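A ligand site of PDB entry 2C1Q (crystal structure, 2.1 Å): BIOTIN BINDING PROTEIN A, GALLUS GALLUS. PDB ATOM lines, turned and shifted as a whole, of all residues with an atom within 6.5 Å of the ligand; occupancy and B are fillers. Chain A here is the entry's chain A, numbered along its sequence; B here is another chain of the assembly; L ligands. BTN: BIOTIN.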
ATOM      1  N   ASN A  13      -6.468  -0.765   8.103  1.00  0.00           N
ATOM      2  CA  ASN A  13      -7.848  -0.552   8.549  1.00  0.00           C
ATOM      3  C   ASN A  13      -8.068   0.862   9.061  1.00  0.00           C
ATOM      4  O   ASN A  13      -7.118   1.660   9.116  1.00  0.00           O
ATOM      5  CB  ASN A  13      -8.309  -1.672   9.507  1.00  0.00           C
ATOM      6  CG  ASN A  13      -7.674  -1.587  10.881  1.00  0.00           C
ATOM      7  OD1 ASN A  13      -7.178  -0.543  11.256  1.00  0.00           O
ATOM      8  ND2 ASN A  13      -7.741  -2.676  11.655  1.00  0.00           N
ATOM      9  N   LEU A  15      -8.495   1.999  11.898  1.00  0.00           N
ATOM     10  CA  LEU A  15      -7.750   2.313  13.120  1.00  0.00           C
ATOM     11  C   LEU A  15      -6.312   2.650  12.789  1.00  0.00           C
ATOM     12  O   LEU A  15      -5.554   3.068  13.655  1.00  0.00           O
ATOM     13  CB  LEU A  15      -7.745   1.133  14.095  1.00  0.00           C
ATOM     14  CG  LEU A  15      -9.079   0.703  14.692  1.00  0.00           C
ATOM     15  CD1 LEU A  15      -8.933  -0.554  15.532  1.00  0.00           C
ATOM     16  CD2 LEU A  15      -9.723   1.830  15.484  1.00  0.00           C
ATOM     17  N   GLY A  16      -5.927   2.426  11.535  1.00  0.00           N
ATOM     18  CA  GLY A  16      -4.550   2.630  11.107  1.00  0.00           C
ATOM     19  C   GLY A  16      -3.675   1.408  11.349  1.00  0.00           C
ATOM     20  O   GLY A  16      -2.447   1.493  11.283  1.00  0.00           O
ATOM     21  N   SER A  17      -4.289   0.252  11.612  1.00  0.00           N
ATOM     22  CA  SER A  17      -3.528  -0.989  11.711  1.00  0.00           C
ATOM     23  C   SER A  17      -3.051  -1.440  10.346  1.00  0.00           C
ATOM     24  O   SER A  17      -3.750  -1.228   9.346  1.00  0.00           O
ATOM     25  CB  SER A  17      -4.392  -2.094  12.333  1.00  0.00           C
ATOM     26  OG  SER A  17      -4.646  -1.824  13.701  1.00  0.00           O
ATOM     27  N   ASN A  18      -1.887  -2.085  10.309  1.00  0.00           N
ATOM     28  CA  ASN A  18      -1.395  -2.705   9.086  1.00  0.00           C
ATOM     29  C   ASN A  18      -1.384  -4.215   9.192  1.00  0.00           C
ATOM     30  O   ASN A  18      -1.071  -4.797  10.249  1.00  0.00           O
ATOM     31  CB  ASN A  18       0.015  -2.200   8.739  1.00  0.00           C
ATOM     32  CG  ASN A  18       0.039  -0.715   8.482  1.00  0.00           C
ATOM     33  OD1 ASN A  18      -0.402  -0.251   7.431  1.00  0.00           O
ATOM     34  ND2 ASN A  18       0.509   0.043   9.468  1.00  0.00           N
ATOM     35  N   TYR A  34       0.546  -8.890  11.435  1.00  0.00           N
ATOM     36  CA  TYR A  34      -0.378  -7.850  11.777  1.00  0.00           C
ATOM     37  C   TYR A  34       0.344  -6.856  12.644  1.00  0.00           C
ATOM     38  O   TYR A  34       0.920  -7.216  13.672  1.00  0.00           O
ATOM     39  CB  TYR A  34      -1.546  -8.438  12.590  1.00  0.00           C
ATOM     40  CG  TYR A  34      -2.814  -7.639  12.510  1.00  0.00           C
ATOM     41  CD1 TYR A  34      -3.796  -7.954  11.562  1.00  0.00           C
ATOM     42  CD2 TYR A  34      -3.045  -6.574  13.369  1.00  0.00           C
ATOM     43  CE1 TYR A  34      -4.990  -7.206  11.487  1.00  0.00           C
ATOM     44  CE2 TYR A  34      -4.236  -5.829  13.303  1.00  0.00           C
ATOM     45  CZ  TYR A  34      -5.173  -6.141  12.363  1.00  0.00           C
ATOM     46  OH  TYR A  34      -6.316  -5.405  12.300  1.00  0.00           O
ATOM     47  N   GLN A  35       0.259  -5.591  12.258  1.00  0.00           N
ATOM     48  CA  GLN A  35       0.772  -4.484  13.084  1.00  0.00           C
ATOM     49  C   GLN A  35      -0.392  -3.605  13.575  1.00  0.00           C
ATOM     50  O   GLN A  35      -0.888  -2.759  12.834  1.00  0.00           O
ATOM     51  CB  GLN A  35       1.734  -3.652  12.270  1.00  0.00           C
ATOM     52  CG  GLN A  35       2.323  -2.459  13.033  1.00  0.00           C
ATOM     53  CD  GLN A  35       3.364  -2.911  14.014  1.00  0.00           C
ATOM     54  OE1 GLN A  35       4.134  -3.823  13.738  1.00  0.00           O
ATOM     55  NE2 GLN A  35       3.382  -2.289  15.182  1.00  0.00           N
ATOM     56  N   THR A  36      -0.849  -3.805  14.801  1.00  0.00           N
ATOM     57  CA  THR A  36      -2.000  -3.057  15.281  1.00  0.00           C
ATOM     58  C   THR A  36      -1.548  -1.678  15.674  1.00  0.00           C
ATOM     59  O   THR A  36      -0.467  -1.524  16.214  1.00  0.00           O
ATOM     60  CB  THR A  36      -2.728  -3.737  16.448  1.00  0.00           C
ATOM     61  OG1 THR A  36      -3.773  -2.879  16.917  1.00  0.00           O
ATOM     62  CG2 THR A  36      -1.793  -3.981  17.614  1.00  0.00           C
ATOM     63  N   ALA A  37      -2.391  -0.688  15.438  1.00  0.00           N
ATOM     64  CA  ALA A  37      -2.109   0.675  15.849  1.00  0.00           C
ATOM     65  C   ALA A  37      -2.531   0.899  17.280  1.00  0.00           C
ATOM     66  O   ALA A  37      -2.122   1.863  17.889  1.00  0.00           O
ATOM     67  CB  ALA A  37      -2.813   1.680  14.938  1.00  0.00           C
ATOM     68  N   VAL A  38      -3.328  -0.040  17.822  1.00  0.00           N
ATOM     69  CA  VAL A  38      -3.955   0.155  19.124  1.00  0.00           C
ATOM     70  C   VAL A  38      -3.801  -1.086  20.010  1.00  0.00           C
ATOM     71  O   VAL A  38      -3.669  -2.220  19.524  1.00  0.00           O
ATOM     72  CB  VAL A  38      -5.472   0.572  18.976  1.00  0.00           C
ATOM     73  CG1 VAL A  38      -5.643   1.969  18.285  1.00  0.00           C
ATOM     74  CG2 VAL A  38      -6.228  -0.478  18.190  1.00  0.00           C
ATOM     75  N   THR A  39      -3.845  -0.897  21.307  1.00  0.00           N
ATOM     76  CA  THR A  39      -3.813  -2.039  22.186  1.00  0.00           C
ATOM     77  C   THR A  39      -4.631  -1.717  23.413  1.00  0.00           C
ATOM     78  O   THR A  39      -4.813  -0.560  23.726  1.00  0.00           O
ATOM     79  CB  THR A  39      -2.372  -2.430  22.530  1.00  0.00           C
ATOM     80  OG1 THR A  39      -2.389  -3.530  23.460  1.00  0.00           O
ATOM     81  CG2 THR A  39      -1.607  -1.250  23.144  1.00  0.00           C
ATOM     82  N   ALA A  40      -5.147  -2.753  24.087  1.00  0.00           N
ATOM     83  CA  ALA A  40      -5.870  -2.573  25.350  1.00  0.00           C
ATOM     84  C   ALA A  40      -4.953  -2.818  26.532  1.00  0.00           C
ATOM     85  O   ALA A  40      -5.377  -2.730  27.681  1.00  0.00           O
ATOM     86  CB  ALA A  40      -7.068  -3.500  25.412  1.00  0.00           C
ATOM     87  N   THR A  41      -3.699  -3.126  26.240  1.00  0.00           N
ATOM     88  CA  THR A  41      -2.691  -3.302  27.282  1.00  0.00           C
ATOM     89  C   THR A  41      -1.861  -2.043  27.374  1.00  0.00           C
ATOM     90  O   THR A  41      -2.048  -1.104  26.582  1.00  0.00           O
ATOM     91  CB  THR A  41      -1.754  -4.466  26.996  1.00  0.00           C
ATOM     92  OG1 THR A  41      -0.977  -4.152  25.833  1.00  0.00           O
ATOM     93  CG2 THR A  41      -2.528  -5.766  26.764  1.00  0.00           C
ATOM     94  N   ILE A  45       3.504  -2.259  21.531  1.00  0.00           N
ATOM     95  CA  ILE A  45       3.031  -3.027  20.379  1.00  0.00           C
ATOM     96  C   ILE A  45       4.189  -3.618  19.539  1.00  0.00           C
ATOM     97  O   ILE A  45       5.135  -2.912  19.228  1.00  0.00           O
ATOM     98  CB  ILE A  45       2.158  -2.160  19.470  1.00  0.00           C
ATOM     99  CG1 ILE A  45       0.844  -1.793  20.193  1.00  0.00           C
ATOM    100  CG2 ILE A  45       1.848  -2.921  18.168  1.00  0.00           C
ATOM    101  CD1 ILE A  45       0.159  -0.574  19.670  1.00  0.00           C
ATOM    102  N   TRP A  72      -0.748 -12.451  19.318  1.00  0.00           N
ATOM    103  CA  TRP A  72      -0.067 -11.207  19.694  1.00  0.00           C
ATOM    104  C   TRP A  72       1.260 -11.458  20.392  1.00  0.00           C
ATOM    105  O   TRP A  72       1.322 -12.235  21.339  1.00  0.00           O
ATOM    106  CB  TRP A  72      -0.966 -10.311  20.565  1.00  0.00           C
ATOM    107  CG  TRP A  72      -2.252  -9.978  19.868  1.00  0.00           C
ATOM    108  CD1 TRP A  72      -3.496 -10.462  20.179  1.00  0.00           C
ATOM    109  CD2 TRP A  72      -2.414  -9.152  18.716  1.00  0.00           C
ATOM    110  NE1 TRP A  72      -4.422  -9.977  19.302  1.00  0.00           N
ATOM    111  CE2 TRP A  72      -3.796  -9.148  18.399  1.00  0.00           C
ATOM    112  CE3 TRP A  72      -1.540  -8.348  17.944  1.00  0.00           C
ATOM    113  CZ2 TRP A  72      -4.316  -8.432  17.330  1.00  0.00           C
ATOM    114  CZ3 TRP A  72      -2.065  -7.629  16.888  1.00  0.00           C
ATOM    115  CH2 TRP A  72      -3.453  -7.672  16.592  1.00  0.00           C
ATOM    116  N   PHE A  74       3.080  -9.397  22.201  1.00  0.00           N
ATOM    117  CA  PHE A  74       3.340  -8.515  23.326  1.00  0.00           C
ATOM    118  C   PHE A  74       2.203  -8.553  24.351  1.00  0.00           C
ATOM    119  O   PHE A  74       2.161  -7.749  25.276  1.00  0.00           O
ATOM    120  CB  PHE A  74       3.475  -7.099  22.794  1.00  0.00           C
ATOM    121  CG  PHE A  74       2.234  -6.612  22.064  1.00  0.00           C
ATOM    122  CD1 PHE A  74       1.215  -5.948  22.749  1.00  0.00           C
ATOM    123  CD2 PHE A  74       2.085  -6.856  20.692  1.00  0.00           C
ATOM    124  CE1 PHE A  74       0.050  -5.505  22.069  1.00  0.00           C
ATOM    125  CE2 PHE A  74       0.939  -6.416  20.026  1.00  0.00           C
ATOM    126  CZ  PHE A  74      -0.075  -5.743  20.712  1.00  0.00           C
ATOM    127  N   ALA A  75       1.249  -9.459  24.154  1.00  0.00           N
ATOM    128  CA  ALA A  75       0.061  -9.509  24.995  1.00  0.00           C
ATOM    129  C   ALA A  75      -0.355 -10.946  25.196  1.00  0.00           C
ATOM    130  O   ALA A  75      -0.119 -11.781  24.330  1.00  0.00           O
ATOM    131  CB  ALA A  75      -1.066  -8.716  24.343  1.00  0.00           C
ATOM    132  N   ASP A  76      -0.978 -11.232  26.340  1.00  0.00           N
ATOM    133  CA  ASP A  76      -1.484 -12.585  26.585  1.00  0.00           C
ATOM    134  C   ASP A  76      -2.732 -12.945  25.786  1.00  0.00           C
ATOM    135  O   ASP A  76      -3.200 -14.076  25.823  1.00  0.00           O
ATOM    136  CB  ASP A  76      -1.693 -12.822  28.080  1.00  0.00           C
ATOM    137  CG  ASP A  76      -0.376 -12.973  28.833  1.00  0.00           C
ATOM    138  OD1 ASP A  76       0.666 -13.187  28.145  1.00  0.00           O
ATOM    139  OD2 ASP A  76      -0.378 -12.883  30.086  1.00  0.00           O
ATOM    140  N   SER A  77      -3.217 -12.017  24.989  1.00  0.00           N
ATOM    141  CA  SER A  77      -4.482 -12.203  24.313  1.00  0.00           C
ATOM    142  C   SER A  77      -4.382 -12.879  22.937  1.00  0.00           C
ATOM    143  O   SER A  77      -3.289 -13.182  22.458  1.00  0.00           O
ATOM    144  CB  SER A  77      -5.100 -10.827  24.166  1.00  0.00           C
ATOM    145  OG  SER A  77      -4.231 -10.054  23.375  1.00  0.00           O
ATOM    146  N   THR A  78      -5.543 -13.130  22.318  1.00  0.00           N
ATOM    147  CA  THR A  78      -5.626 -13.681  20.985  1.00  0.00           C
ATOM    148  C   THR A  78      -6.814 -13.025  20.289  1.00  0.00           C
ATOM    149  O   THR A  78      -7.872 -12.902  20.888  1.00  0.00           O
ATOM    150  CB  THR A  78      -5.798 -15.216  21.023  1.00  0.00           C
ATOM    151  OG1 THR A  78      -4.658 -15.821  21.662  1.00  0.00           O
ATOM    152  CG2 THR A  78      -5.858 -15.743  19.656  1.00  0.00           C
ATOM    153  N   THR A  79      -6.620 -12.554  19.067  1.00  0.00           N
ATOM    154  CA  THR A  79      -7.739 -12.049  18.270  1.00  0.00           C
ATOM    155  C   THR A  79      -8.003 -12.963  17.104  1.00  0.00           C
ATOM    156  O   THR A  79      -7.064 -13.465  16.482  1.00  0.00           O
ATOM    157  CB  THR A  79      -7.515 -10.633  17.709  1.00  0.00           C
ATOM    158  OG1 THR A  79      -7.281  -9.729  18.783  1.00  0.00           O
ATOM    159  CG2 THR A  79      -8.787 -10.137  16.981  1.00  0.00           C
ATOM    160  N   PHE A  81     -10.291 -12.921  13.394  1.00  0.00           N
ATOM    161  CA  PHE A  81     -10.970 -11.985  12.519  1.00  0.00           C
ATOM    162  C   PHE A  81     -11.674 -12.858  11.508  1.00  0.00           C
ATOM    163  O   PHE A  81     -11.124 -13.848  11.061  1.00  0.00           O
ATOM    164  CB  PHE A  81      -9.951 -11.186  11.753  1.00  0.00           C
ATOM    165  CG  PHE A  81      -9.341 -10.042  12.494  1.00  0.00           C
ATOM    166  CD1 PHE A  81      -9.789  -8.729  12.251  1.00  0.00           C
ATOM    167  CD2 PHE A  81      -8.241 -10.244  13.346  1.00  0.00           C
ATOM    168  CE1 PHE A  81      -9.185  -7.624  12.905  1.00  0.00           C
ATOM    169  CE2 PHE A  81      -7.619  -9.162  13.987  1.00  0.00           C
ATOM    170  CZ  PHE A  81      -8.095  -7.831  13.770  1.00  0.00           C
ATOM    171  N   TRP A  99     -14.452  -9.261  14.520  1.00  0.00           N
ATOM    172  CA  TRP A  99     -13.379  -9.842  15.298  1.00  0.00           C
ATOM    173  C   TRP A  99     -13.759 -10.028  16.754  1.00  0.00           C
ATOM    174  O   TRP A  99     -14.682  -9.405  17.253  1.00  0.00           O
ATOM    175  CB  TRP A  99     -12.104  -8.979  15.191  1.00  0.00           C
ATOM    176  CG  TRP A  99     -12.246  -7.515  15.616  1.00  0.00           C
ATOM    177  CD1 TRP A  99     -12.308  -6.427  14.774  1.00  0.00           C
ATOM    178  CD2 TRP A  99     -12.280  -6.982  16.971  1.00  0.00           C
ATOM    179  NE1 TRP A  99     -12.398  -5.258  15.520  1.00  0.00           N
ATOM    180  CE2 TRP A  99     -12.390  -5.573  16.855  1.00  0.00           C
ATOM    181  CE3 TRP A  99     -12.246  -7.558  18.262  1.00  0.00           C
ATOM    182  CZ2 TRP A  99     -12.478  -4.740  17.979  1.00  0.00           C
ATOM    183  CZ3 TRP A  99     -12.294  -6.725  19.363  1.00  0.00           C
ATOM    184  CH2 TRP A  99     -12.421  -5.328  19.227  1.00  0.00           C
ATOM    185  N   LEU A 100     -13.047 -10.934  17.408  1.00  0.00           N
ATOM    186  CA  LEU A 100     -13.170 -11.154  18.847  1.00  0.00           C
ATOM    187  C   LEU A 100     -11.773 -11.114  19.435  1.00  0.00           C
ATOM    188  O   LEU A 100     -10.879 -11.792  18.950  1.00  0.00           O
ATOM    189  CB  LEU A 100     -13.772 -12.519  19.174  1.00  0.00           C
ATOM    190  CG  LEU A 100     -15.199 -12.826  18.690  1.00  0.00           C
ATOM    191  CD1 LEU A 100     -15.504 -14.327  18.857  1.00  0.00           C
ATOM    192  CD2 LEU A 100     -16.248 -11.983  19.395  1.00  0.00           C
ATOM    193  N   LEU A 101     -11.598 -10.312  20.476  1.00  0.00           N
ATOM    194  CA  LEU A 101     -10.315 -10.238  21.155  1.00  0.00           C
ATOM    195  C   LEU A 101     -10.494 -10.912  22.485  1.00  0.00           C
ATOM    196  O   LEU A 101     -11.324 -10.498  23.274  1.00  0.00           O
ATOM    197  CB  LEU A 101      -9.908  -8.787  21.344  1.00  0.00           C
ATOM    198  CG  LEU A 101      -8.805  -8.427  22.365  1.00  0.00           C
ATOM    199  CD1 LEU A 101      -7.515  -9.168  22.116  1.00  0.00           C
ATOM    200  CD2 LEU A 101      -8.520  -6.907  22.286  1.00  0.00           C
ATOM    201  N   ARG A 102      -9.689 -11.938  22.744  1.00  0.00           N
ATOM    202  CA  ARG A 102      -9.829 -12.752  23.953  1.00  0.00           C
ATOM    203  C   ARG A 102      -8.640 -12.506  24.858  1.00  0.00           C
ATOM    204  O   ARG A 102      -7.519 -12.837  24.492  1.00  0.00           O
ATOM    205  CB  ARG A 102      -9.824 -14.234  23.589  1.00  0.00           C
ATOM    206  CG  ARG A 102      -9.925 -15.211  24.802  1.00  0.00           C
ATOM    207  CD  ARG A 102     -11.332 -15.390  25.018  1.00  0.00           C
ATOM    208  NE  ARG A 102     -11.751 -16.302  26.069  1.00  0.00           N
ATOM    209  CZ  ARG A 102     -12.922 -16.917  25.988  1.00  0.00           C
ATOM    210  NH1 ARG A 102     -13.670 -16.736  24.884  1.00  0.00           N
ATOM    211  NH2 ARG A 102     -13.335 -17.705  26.943  1.00  0.00           N
ATOM    212  N   GLU A 103      -8.892 -11.916  26.027  1.00  0.00           N
ATOM    213  CA  GLU A 103      -7.850 -11.769  27.025  1.00  0.00           C
ATOM    214  C   GLU A 103      -7.714 -13.021  27.892  1.00  0.00           C
ATOM    215  O   GLU A 103      -8.689 -13.706  28.196  1.00  0.00           O
ATOM    216  CB  GLU A 103      -8.019 -10.477  27.867  1.00  0.00           C
ATOM    217  CG  GLU A 103      -8.136  -9.210  26.944  1.00  0.00           C
ATOM    218  CD  GLU A 103      -7.136  -8.098  27.243  1.00  0.00           C
ATOM    219  OE1 GLU A 103      -7.304  -7.423  28.290  1.00  0.00           O
ATOM    220  OE2 GLU A 103      -6.187  -7.858  26.428  1.00  0.00           O
ATOM    221  N   THR A 119     -15.743  -4.511  14.719  1.00  0.00           N
ATOM    222  CA  THR A 119     -15.569  -4.707  13.279  1.00  0.00           C
ATOM    223  C   THR A 119     -14.395  -3.866  12.782  1.00  0.00           C
ATOM    224  O   THR A 119     -13.989  -2.916  13.454  1.00  0.00           O
ATOM    225  CB  THR A 119     -16.871  -4.310  12.520  1.00  0.00           C
ATOM    226  OG1 THR A 119     -17.251  -2.993  12.901  1.00  0.00           O
ATOM    227  CG2 THR A 119     -18.061  -5.264  12.878  1.00  0.00           C
ATOM    228  N   ASN A 120     -13.841  -4.215  11.610  1.00  0.00           N
ATOM    229  CA  ASN A 120     -12.808  -3.385  10.959  1.00  0.00           C
ATOM    230  C   ASN A 120     -13.080  -3.373   9.453  1.00  0.00           C
ATOM    231  O   ASN A 120     -13.708  -4.288   8.940  1.00  0.00           O
ATOM    232  CB  ASN A 120     -11.391  -3.935  11.208  1.00  0.00           C
ATOM    233  CG  ASN A 120     -10.826  -3.516  12.552  1.00  0.00           C
ATOM    234  OD1 ASN A 120     -10.096  -4.274  13.202  1.00  0.00           O
ATOM    235  ND2 ASN A 120     -11.110  -2.294  12.962  1.00  0.00           N
ATOM    236  N   PHE A 122     -10.820  -2.944   5.962  1.00  0.00           N
ATOM    237  CA  PHE A 122      -9.444  -2.819   5.455  1.00  0.00           C
ATOM    238  C   PHE A 122      -9.459  -2.416   3.996  1.00  0.00           C
ATOM    239  O   PHE A 122     -10.291  -2.899   3.222  1.00  0.00           O
ATOM    240  CB  PHE A 122      -8.651  -4.132   5.554  1.00  0.00           C
ATOM    241  CG  PHE A 122      -8.410  -4.616   6.948  1.00  0.00           C
ATOM    242  CD1 PHE A 122      -7.156  -4.524   7.522  1.00  0.00           C
ATOM    243  CD2 PHE A 122      -9.426  -5.206   7.678  1.00  0.00           C
ATOM    244  CE1 PHE A 122      -6.921  -5.019   8.794  1.00  0.00           C
ATOM    245  CE2 PHE A 122      -9.210  -5.651   8.950  1.00  0.00           C
ATOM    246  CZ  PHE A 122      -7.956  -5.583   9.505  1.00  0.00           C
ATOM    247  N   TRP B 112     -12.975   1.155  19.791  1.00  0.00           N
ATOM    248  CA  TRP B 112     -12.722  -0.225  19.322  1.00  0.00           C
ATOM    249  C   TRP B 112     -12.709  -1.263  20.457  1.00  0.00           C
ATOM    250  O   TRP B 112     -13.089  -2.401  20.246  1.00  0.00           O
ATOM    251  CB  TRP B 112     -11.417  -0.344  18.491  1.00  0.00           C
ATOM    252  CG  TRP B 112     -10.207  -0.270  19.379  1.00  0.00           C
ATOM    253  CD1 TRP B 112      -9.534   0.869  19.770  1.00  0.00           C
ATOM    254  CD2 TRP B 112      -9.543  -1.362  20.025  1.00  0.00           C
ATOM    255  NE1 TRP B 112      -8.512   0.550  20.622  1.00  0.00           N
ATOM    256  CE2 TRP B 112      -8.489  -0.814  20.791  1.00  0.00           C
ATOM    257  CE3 TRP B 112      -9.736  -2.768  20.010  1.00  0.00           C
ATOM    258  CZ2 TRP B 112      -7.634  -1.619  21.539  1.00  0.00           C
ATOM    259  CZ3 TRP B 112      -8.896  -3.552  20.780  1.00  0.00           C
ATOM    260  CH2 TRP B 112      -7.852  -2.983  21.523  1.00  0.00           C
HETATM  261  C11 BTN L   1      -4.338  -6.584  22.856  1.00  0.00           C
HETATM  262  O11 BTN L   1      -4.475  -7.417  23.797  1.00  0.00           O
HETATM  263  O12 BTN L   1      -4.657  -5.396  23.069  1.00  0.00           O
HETATM  264  C10 BTN L   1      -3.754  -6.976  21.497  1.00  0.00           C
HETATM  265  C9  BTN L   1      -3.910  -5.869  20.451  1.00  0.00           C
HETATM  266  C8  BTN L   1      -5.290  -6.085  19.793  1.00  0.00           C
HETATM  267  C7  BTN L   1      -5.665  -5.011  18.797  1.00  0.00           C
HETATM  268  C2  BTN L   1      -7.124  -5.164  18.358  1.00  0.00           C
HETATM  269  S1  BTN L   1      -7.434  -6.594  17.477  1.00  0.00           S
HETATM  270  C6  BTN L   1      -8.969  -5.874  16.891  1.00  0.00           C
HETATM  271  C5  BTN L   1      -8.822  -4.386  16.738  1.00  0.00           C
HETATM  272  N1  BTN L   1      -8.459  -4.169  15.362  1.00  0.00           N
HETATM  273  C3  BTN L   1      -7.193  -3.791  15.275  1.00  0.00           C
HETATM  274  O3  BTN L   1      -6.603  -3.512  14.052  1.00  0.00           O
HETATM  275  N2  BTN L   1      -6.603  -3.708  16.466  1.00  0.00           N
HETATM  276  C4  BTN L   1      -7.554  -3.977  17.513  1.00  0.00           C
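An oxygen (O11) of the ligand sits close to the side-chain carboxylate (OE2) of Glu 103. Residues that only touch the ligand: Leu 15, Val 38, Thr 41, Trp 72, Phe 74, Ala 75, Phe 81, Trp 99, Leu 101 and Trp 112 of chain B. Hydrophobic or aromatic side chains that line the ligand: Leu 15, Tyr 34, Val 38, Ala 40, Trp 72, Phe 74, Ala 75, Phe 81, Trp 99, Leu 101 and Trp 112 of chain B. Within 4 Å of the ligand: Asn 13, Leu 15, Ser 17, Tyr 34, Thr 36, Val 38, Thr 39, Ala 40, Thr 41, Trp 72, Phe 74, Ala 75, Ser 77, Thr 79, Phe 81, Trp 99, Leu 101, Glu 103, Asn 120 and Trp 112 of chain B.
OH of Tyr 34 is in hydrogen-bond range of O3 of the ligand. The side-chain hydroxyl of Ser 17 sits at hydrogen-bond distance from an oxygen (O3) of the ligand (2.6 Å). An oxygen (O11) of the ligand lies within hydrogen-bond range of the side-chain hydroxyl of Ser 77, at 2.7 Å. The side-chain amide oxygen (OD1) of Asn 120 sits at hydrogen-bond distance from a nitrogen (N1) of the ligand. ND2 of Asn 13 sits at hydrogen-bond distance from O3 of the ligand, 2.8 Å away. The backbone NH (N) of Ala 40 sits at hydrogen-bond distance from an oxygen (O12) of the ligand (2.9 Å). OG1 of Thr 39 is in hydrogen-bond range of O12 of the ligand (3.0 Å). The side-chain hydroxyl of Thr 36 lies within hydrogen-bond range of a nitrogen (N2) of the ligand (3.0 Å). S1 of the ligand lies close to OG1 of Thr 79 (3.4 Å).
ND2 of Asn 13 is in hydrogen-bond range of OH of Tyr 34, 3.1 Å away. The side-chain hydroxyl (OG) of Ser 17 sits at hydrogen-bond distance from the backbone NH (N) of Ala 37 (3.1 Å). The side-chain amide oxygen (OD1) of Asn 120 sits at hydrogen-bond distance from the side-chain amide nitrogen (ND2) of Asn 13 (3.2 Å). OD1 of Asn 120 sits at hydrogen-bond distance from NE1 of Trp 99, at 3.4 Å. The side-chain amide oxygen of Asn 13 sits at hydrogen-bond distance from the backbone NH of Leu 15 (2.9 Å). The backbone NH (N) of Gly 16 is in hydrogen-bond range of the side-chain amide oxygen (OD1) of Asn 13 (3.2 Å). The side-chain hydroxyl (OG1) of Thr 36 sits at hydrogen-bond distance from the backbone carbonyl oxygen (O) of Val 38 (2.7 Å). NE1 of Trp 72 is in hydrogen-bond range of OG1 of Thr 79, 2.9 Å away.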
